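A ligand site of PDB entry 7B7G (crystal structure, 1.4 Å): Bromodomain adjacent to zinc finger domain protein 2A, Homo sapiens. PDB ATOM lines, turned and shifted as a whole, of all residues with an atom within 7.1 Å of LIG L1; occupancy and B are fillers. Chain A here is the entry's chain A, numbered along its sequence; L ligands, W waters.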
ATOM      1  N   TRP A  23       9.332  28.726  17.339  1.00  0.00           N
ATOM      2  CA  TRP A  23      10.119  28.739  16.104  1.00  0.00           C
ATOM      3  C   TRP A  23       9.484  28.029  14.921  1.00  0.00           C
ATOM      4  O   TRP A  23       9.647  28.511  13.796  1.00  0.00           O
ATOM      5  CB  TRP A  23      11.564  28.264  16.375  1.00  0.00           C
ATOM      6  CG  TRP A  23      11.686  26.801  16.747  1.00  0.00           C
ATOM      7  CD1 TRP A  23      11.728  26.280  18.012  1.00  0.00           C
ATOM      8  CD2 TRP A  23      11.733  25.683  15.845  1.00  0.00           C
ATOM      9  NE1 TRP A  23      11.793  24.895  17.946  1.00  0.00           N
ATOM     10  CE2 TRP A  23      11.793  24.515  16.621  1.00  0.00           C
ATOM     11  CE3 TRP A  23      11.709  25.578  14.455  1.00  0.00           C
ATOM     12  CZ2 TRP A  23      11.859  23.240  16.053  1.00  0.00           C
ATOM     13  CZ3 TRP A  23      11.769  24.315  13.887  1.00  0.00           C
ATOM     14  CH2 TRP A  23      11.842  23.161  14.689  1.00  0.00           C
ATOM     15  N   PRO A  24       8.778  26.895  15.067  1.00  0.00           N
ATOM     16  CA  PRO A  24       8.220  26.265  13.865  1.00  0.00           C
ATOM     17  C   PRO A  24       7.094  27.053  13.238  1.00  0.00           C
ATOM     18  O   PRO A  24       6.710  26.754  12.093  1.00  0.00           O
ATOM     19  CB  PRO A  24       7.700  24.901  14.378  1.00  0.00           C
ATOM     20  CG  PRO A  24       8.332  24.692  15.692  1.00  0.00           C
ATOM     21  CD  PRO A  24       8.515  26.077  16.269  1.00  0.00           C
ATOM     22  N   PHE A  25       6.528  28.011  13.976  1.00  0.00           N
ATOM     23  CA  PHE A  25       5.246  28.626  13.637  1.00  0.00           C
ATOM     24  C   PHE A  25       5.353  30.105  13.331  1.00  0.00           C
ATOM     25  O   PHE A  25       4.324  30.747  13.103  1.00  0.00           O
ATOM     26  CB  PHE A  25       4.268  28.412  14.792  1.00  0.00           C
ATOM     27  CG  PHE A  25       4.281  27.020  15.321  1.00  0.00           C
ATOM     28  CD1 PHE A  25       3.873  25.950  14.521  1.00  0.00           C
ATOM     29  CD2 PHE A  25       4.720  26.750  16.625  1.00  0.00           C
ATOM     30  CE1 PHE A  25       3.913  24.661  14.996  1.00  0.00           C
ATOM     31  CE2 PHE A  25       4.767  25.448  17.099  1.00  0.00           C
ATOM     32  CZ  PHE A  25       4.377  24.402  16.287  1.00  0.00           C
ATOM     33  N   LEU A  26       6.566  30.666  13.255  1.00  0.00           N
ATOM     34  CA  LEU A  26       6.717  32.105  13.110  1.00  0.00           C
ATOM     35  C   LEU A  26       6.329  32.581  11.714  1.00  0.00           C
ATOM     36  O   LEU A  26       5.795  33.681  11.564  1.00  0.00           O
ATOM     37  CB  LEU A  26       8.159  32.533  13.419  1.00  0.00           C
ATOM     38  CG  LEU A  26       8.609  32.285  14.861  1.00  0.00           C
ATOM     39  CD1 LEU A  26      10.066  32.655  14.981  1.00  0.00           C
ATOM     40  CD2 LEU A  26       7.784  33.055  15.847  1.00  0.00           C
ATOM     41  N   GLU A  27       6.586  31.770  10.703  1.00  0.00           N
ATOM     42  CA  GLU A  27       6.324  32.093   9.312  1.00  0.00           C
ATOM     43  C   GLU A  27       5.632  30.932   8.657  1.00  0.00           C
ATOM     44  O   GLU A  27       5.625  29.809   9.192  1.00  0.00           O
ATOM     45  CB  GLU A  27       7.638  32.382   8.570  1.00  0.00           C
ATOM     46  CG  GLU A  27       8.463  33.523   9.138  1.00  0.00           C
ATOM     47  CD  GLU A  27       9.746  33.736   8.358  1.00  0.00           C
ATOM     48  OE1 GLU A  27       9.676  34.231   7.216  1.00  0.00           O
ATOM     49  OE2 GLU A  27      10.832  33.384   8.868  1.00  0.00           O
ATOM     50  N   PRO A  28       5.006  31.137   7.496  1.00  0.00           N
ATOM     51  CA  PRO A  28       4.343  30.012   6.813  1.00  0.00           C
ATOM     52  C   PRO A  28       5.286  28.825   6.664  1.00  0.00           C
ATOM     53  O   PRO A  28       6.498  28.976   6.461  1.00  0.00           O
ATOM     54  CB  PRO A  28       3.986  30.595   5.445  1.00  0.00           C
ATOM     55  CG  PRO A  28       3.869  32.075   5.689  1.00  0.00           C
ATOM     56  CD  PRO A  28       4.888  32.404   6.746  1.00  0.00           C
ATOM     57  N   VAL A  29       4.737  27.613   6.754  1.00  0.00           N
ATOM     58  CA  VAL A  29       5.551  26.430   6.510  1.00  0.00           C
ATOM     59  C   VAL A  29       6.157  26.555   5.124  1.00  0.00           C
ATOM     60  O   VAL A  29       5.461  26.808   4.136  1.00  0.00           O
ATOM     61  CB  VAL A  29       4.746  25.129   6.661  1.00  0.00           C
ATOM     62  CG1 VAL A  29       5.608  23.919   6.254  1.00  0.00           C
ATOM     63  CG2 VAL A  29       4.252  24.993   8.105  1.00  0.00           C
ATOM     64  N   ASN A  30       7.476  26.360   5.052  1.00  0.00           N
ATOM     65  CA  ASN A  30       8.274  26.788   3.917  1.00  0.00           C
ATOM     66  C   ASN A  30       8.560  25.604   3.007  1.00  0.00           C
ATOM     67  O   ASN A  30       9.285  24.684   3.419  1.00  0.00           O
ATOM     68  CB  ASN A  30       9.573  27.357   4.486  1.00  0.00           C
ATOM     69  CG  ASN A  30      10.466  27.998   3.459  1.00  0.00           C
ATOM     70  OD1 ASN A  30      10.315  27.824   2.245  1.00  0.00           O
ATOM     71  ND2 ASN A  30      11.465  28.735   3.950  1.00  0.00           N
ATOM     72  N   LEU A  33      11.951  24.000   2.801  1.00  0.00           N
ATOM     73  CA  LEU A  33      12.444  23.242   3.947  1.00  0.00           C
ATOM     74  C   LEU A  33      11.589  22.038   4.318  1.00  0.00           C
ATOM     75  O   LEU A  33      12.099  21.120   4.972  1.00  0.00           O
ATOM     76  CB  LEU A  33      12.510  24.152   5.188  1.00  0.00           C
ATOM     77  CG  LEU A  33      13.359  25.409   5.001  1.00  0.00           C
ATOM     78  CD1 LEU A  33      13.294  26.277   6.266  1.00  0.00           C
ATOM     79  CD2 LEU A  33      14.797  25.054   4.628  1.00  0.00           C
ATOM     80  N   VAL A  34      10.310  22.013   3.945  1.00  0.00           N
ATOM     81  CA  VAL A  34       9.372  20.982   4.377  1.00  0.00           C
ATOM     82  C   VAL A  34       8.592  20.571   3.147  1.00  0.00           C
ATOM     83  O   VAL A  34       7.954  21.410   2.516  1.00  0.00           O
ATOM     84  CB  VAL A  34       8.406  21.514   5.451  1.00  0.00           C
ATOM     85  CG1 VAL A  34       7.412  20.436   5.884  1.00  0.00           C
ATOM     86  CG2 VAL A  34       9.169  22.057   6.656  1.00  0.00           C
ATOM     87  N   TYR A  37       3.637  19.549   2.537  1.00  0.00           N
ATOM     88  CA  TYR A  37       2.846  20.120   3.617  1.00  0.00           C
ATOM     89  C   TYR A  37       1.435  20.460   3.156  1.00  0.00           C
ATOM     90  O   TYR A  37       0.456  19.937   3.686  1.00  0.00           O
ATOM     91  CB  TYR A  37       3.563  21.322   4.231  1.00  0.00           C
ATOM     92  CG  TYR A  37       2.860  21.832   5.456  1.00  0.00           C
ATOM     93  CD1 TYR A  37       3.001  21.176   6.670  1.00  0.00           C
ATOM     94  CD2 TYR A  37       2.010  22.949   5.404  1.00  0.00           C
ATOM     95  CE1 TYR A  37       2.333  21.615   7.791  1.00  0.00           C
ATOM     96  CE2 TYR A  37       1.336  23.386   6.518  1.00  0.00           C
ATOM     97  CZ  TYR A  37       1.503  22.733   7.707  1.00  0.00           C
ATOM     98  OH  TYR A  37       0.798  23.187   8.799  1.00  0.00           O
ATOM     99  N   VAL A  72      -3.207  26.946  13.895  1.00  0.00           N
ATOM    100  CA  VAL A  72      -1.764  26.684  13.950  1.00  0.00           C
ATOM    101  C   VAL A  72      -1.517  25.350  14.652  1.00  0.00           C
ATOM    102  O   VAL A  72      -0.774  24.496  14.163  1.00  0.00           O
ATOM    103  CB  VAL A  72      -1.012  27.841  14.637  1.00  0.00           C
ATOM    104  CG1 VAL A  72       0.462  27.500  14.768  1.00  0.00           C
ATOM    105  CG2 VAL A  72      -1.161  29.163  13.849  1.00  0.00           C
ATOM    106  N   ASN A  75      -3.181  22.188  12.827  1.00  0.00           N
ATOM    107  CA  ASN A  75      -2.381  21.799  11.676  1.00  0.00           C
ATOM    108  C   ASN A  75      -1.128  21.064  12.121  1.00  0.00           C
ATOM    109  O   ASN A  75      -0.723  20.068  11.520  1.00  0.00           O
ATOM    110  CB  ASN A  75      -1.997  23.006  10.842  1.00  0.00           C
ATOM    111  CG  ASN A  75      -3.139  23.608  10.079  1.00  0.00           C
ATOM    112  OD1 ASN A  75      -4.177  22.981   9.892  1.00  0.00           O
ATOM    113  ND2 ASN A  75      -2.934  24.819   9.580  1.00  0.00           N
ATOM    114  N   CYS A  76      -0.474  21.580  13.167  1.00  0.00           N
ATOM    115  CA  CYS A  76       0.741  20.953  13.658  1.00  0.00           C
ATOM    116  C   CYS A  76       0.484  19.518  14.085  1.00  0.00           C
ATOM    117  O   CYS A  76       1.275  18.617  13.771  1.00  0.00           O
ATOM    118  CB  CYS A  76       1.300  21.776  14.807  1.00  0.00           C
ATOM    119  SG  CYS A  76       2.868  21.159  15.452  1.00  0.00           S
ATOM    120  N   PHE A  79      -0.006  17.225  10.919  1.00  0.00           N
ATOM    121  CA  PHE A  79       1.136  16.935  10.066  1.00  0.00           C
ATOM    122  C   PHE A  79       2.265  16.226  10.786  1.00  0.00           C
ATOM    123  O   PHE A  79       3.020  15.468  10.146  1.00  0.00           O
ATOM    124  CB  PHE A  79       1.694  18.229   9.491  1.00  0.00           C
ATOM    125  CG  PHE A  79       2.689  18.026   8.381  1.00  0.00           C
ATOM    126  CD1 PHE A  79       2.249  17.655   7.118  1.00  0.00           C
ATOM    127  CD2 PHE A  79       4.056  18.173   8.592  1.00  0.00           C
ATOM    128  CE1 PHE A  79       3.146  17.456   6.098  1.00  0.00           C
ATOM    129  CE2 PHE A  79       4.954  17.966   7.560  1.00  0.00           C
ATOM    130  CZ  PHE A  79       4.492  17.625   6.319  1.00  0.00           C
ATOM    131  N   ASN A  80       2.433  16.455  12.076  1.00  0.00           N
ATOM    132  CA  ASN A  80       3.653  16.072  12.774  1.00  0.00           C
ATOM    133  C   ASN A  80       3.342  15.015  13.821  1.00  0.00           C
ATOM    134  O   ASN A  80       2.309  15.065  14.473  1.00  0.00           O
ATOM    135  CB  ASN A  80       4.298  17.260  13.476  1.00  0.00           C
ATOM    136  CG  ASN A  80       4.632  18.382  12.523  1.00  0.00           C
ATOM    137  OD1 ASN A  80       3.890  19.375  12.382  1.00  0.00           O
ATOM    138  ND2 ASN A  80       5.750  18.246  11.857  1.00  0.00           N
ATOM    139  N   VAL A  86       8.846  19.350  16.228  1.00  0.00           N
ATOM    140  CA  VAL A  86       7.787  20.302  15.913  1.00  0.00           C
ATOM    141  C   VAL A  86       6.482  19.885  16.585  1.00  0.00           C
ATOM    142  O   VAL A  86       5.736  20.738  17.091  1.00  0.00           O
ATOM    143  CB  VAL A  86       7.662  20.452  14.381  1.00  0.00           C
ATOM    144  CG1 VAL A  86       6.451  21.275  14.018  1.00  0.00           C
ATOM    145  CG2 VAL A  86       8.920  21.097  13.813  1.00  0.00           C
ATOM    146  N   GLY A  87       6.187  18.591  16.645  1.00  0.00           N
ATOM    147  CA  GLY A  87       4.985  18.158  17.344  1.00  0.00           C
ATOM    148  C   GLY A  87       4.990  18.572  18.806  1.00  0.00           C
ATOM    149  O   GLY A  87       3.995  19.077  19.319  1.00  0.00           O
HETATM  150  C1  LIG L   1       6.710  22.890  10.630  1.00  0.00           C
HETATM  151  C2  LIG L   1       5.587  23.562  11.062  1.00  0.00           C
HETATM  152  C3  LIG L   1      14.158  26.806  10.838  1.00  0.00           C
HETATM  153  C4  LIG L   1      12.763  27.169  10.340  1.00  0.00           C
HETATM  154  C5  LIG L   1      11.843  25.954  10.261  1.00  0.00           C
HETATM  155  C6  LIG L   1      12.348  24.734   9.834  1.00  0.00           C
HETATM  156  C7  LIG L   1      11.526  23.616   9.752  1.00  0.00           C
HETATM  157  C8  LIG L   1      10.162  23.756  10.089  1.00  0.00           C
HETATM  158  C9  LIG L   1       8.073  23.486  10.486  1.00  0.00           C
HETATM  159  C10 LIG L   1       9.671  24.951  10.500  1.00  0.00           C
HETATM  160  C11 LIG L   1      10.508  26.083  10.590  1.00  0.00           C
HETATM  161  C12 LIG L   1       7.212  20.599   9.869  1.00  0.00           C
HETATM  162  N1  LIG L   1       9.160  22.853  10.085  1.00  0.00           N
HETATM  163  N2  LIG L   1       8.369  24.762  10.747  1.00  0.00           N
HETATM  164  N3  LIG L   1       4.585  22.713  11.050  1.00  0.00           N
HETATM  165  N4  LIG L   1       5.062  21.534  10.602  1.00  0.00           N
HETATM  166  N5  LIG L   1       6.365  21.662  10.353  1.00  0.00           N
HETATM  167  C1  LG2 L   2      16.520  24.466  11.926  1.00  0.00           C
HETATM  168  C2  LG2 L   2      15.722  23.499  11.359  1.00  0.00           C
HETATM  169  C3  LG2 L   2      14.924  22.127   8.080  1.00  0.00           C
HETATM  170  O1  LG2 L   2      17.874  26.063   8.857  1.00  0.00           O
HETATM  171  C4  LG2 L   2      17.236  25.333  11.112  1.00  0.00           C
HETATM  172  C5  LG2 L   2      15.935  23.700  14.374  1.00  0.00           C
HETATM  173  C6  LG2 L   2      15.074  24.378  15.432  1.00  0.00           C
HETATM  174  C7  LG2 L   2      14.782  29.388  18.169  1.00  0.00           C
HETATM  175  C8  LG2 L   2      15.009  27.016  18.040  1.00  0.00           C
HETATM  176  C9  LG2 L   2      14.800  25.630  20.143  1.00  0.00           C
HETATM  177  C10 LG2 L   2      15.441  25.726  15.854  1.00  0.00           C
HETATM  178  C11 LG2 L   2      16.778  26.091  15.459  1.00  0.00           C
HETATM  179  C12 LG2 L   2      16.885  26.026  13.945  1.00  0.00           C
HETATM  180  C13 LG2 L   2      15.666  23.388   9.988  1.00  0.00           C
HETATM  181  C14 LG2 L   2      16.374  24.243   9.172  1.00  0.00           C
HETATM  182  C15 LG2 L   2      17.159  25.220   9.731  1.00  0.00           C
HETATM  183  C16 LG2 L   2      18.459  27.214   9.401  1.00  0.00           C
HETATM  184  N1  LG2 L   2      14.994  28.137  17.455  1.00  0.00           N
HETATM  185  N2  LG2 L   2      14.795  26.925  19.476  1.00  0.00           N
HETATM  186  N3  LG2 L   2      15.235  25.777  17.293  1.00  0.00           N
HETATM  187  N4  LG2 L   2      16.616  24.634  13.366  1.00  0.00           N
HETATM  188  O2  LG2 L   2      14.847  22.396   9.451  1.00  0.00           O
HETATM  189  O   HOH W   1       9.011  25.897   7.462  1.00  0.00           O
HETATM  190  O   HOH W   2      10.865  20.355   9.836  1.00  0.00           O
HETATM  191  O   HOH W   3       1.909  22.652  11.105  1.00  0.00           O
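OD1 of Asn 80 sits close to N4 of LIG L1 (3.0 Å). The backbone carbonyl oxygen (O) of Pro 24 lies close to a nitrogen (N2) of LIG L1 (2.9 Å).
Residues that only touch LIG L1: Val 34 (3.5 Å), Val 29 (3.5 Å), Val 86 (3.7 Å), Tyr 37 (3.9 Å) and Trp 23 (3.9 Å). Hydrophobic or aromatic side chains within 4 Å of LIG L1: Trp 23, Pro 24, Val 29, Val 34, Tyr 37 and Val 86. Within 4 Å of LIG L1: Trp 23, Pro 24, Val 29, Val 34, Tyr 37, Asn 80 and Val 86. The nearest printed residue that does not touch LIG L1 is Leu 33 (4.001 Å).
O of Cys 76 sits close to OD1 of Asn 80, 3.1 Å away. The backbone carbonyl oxygen (O) of Val 86 lies within hydrogen-bond range of the side-chain sulfur (SG) of Cys 76, 3.3 Å away.
Water W3 lies within hydrogen-bond range of the side-chain hydroxyl (OH) of Tyr 37 (2.6 Å), a nitrogen (N3) of LIG L1 (2.7 Å) and the backbone NH (N) of Cys 76 (3.3 Å).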
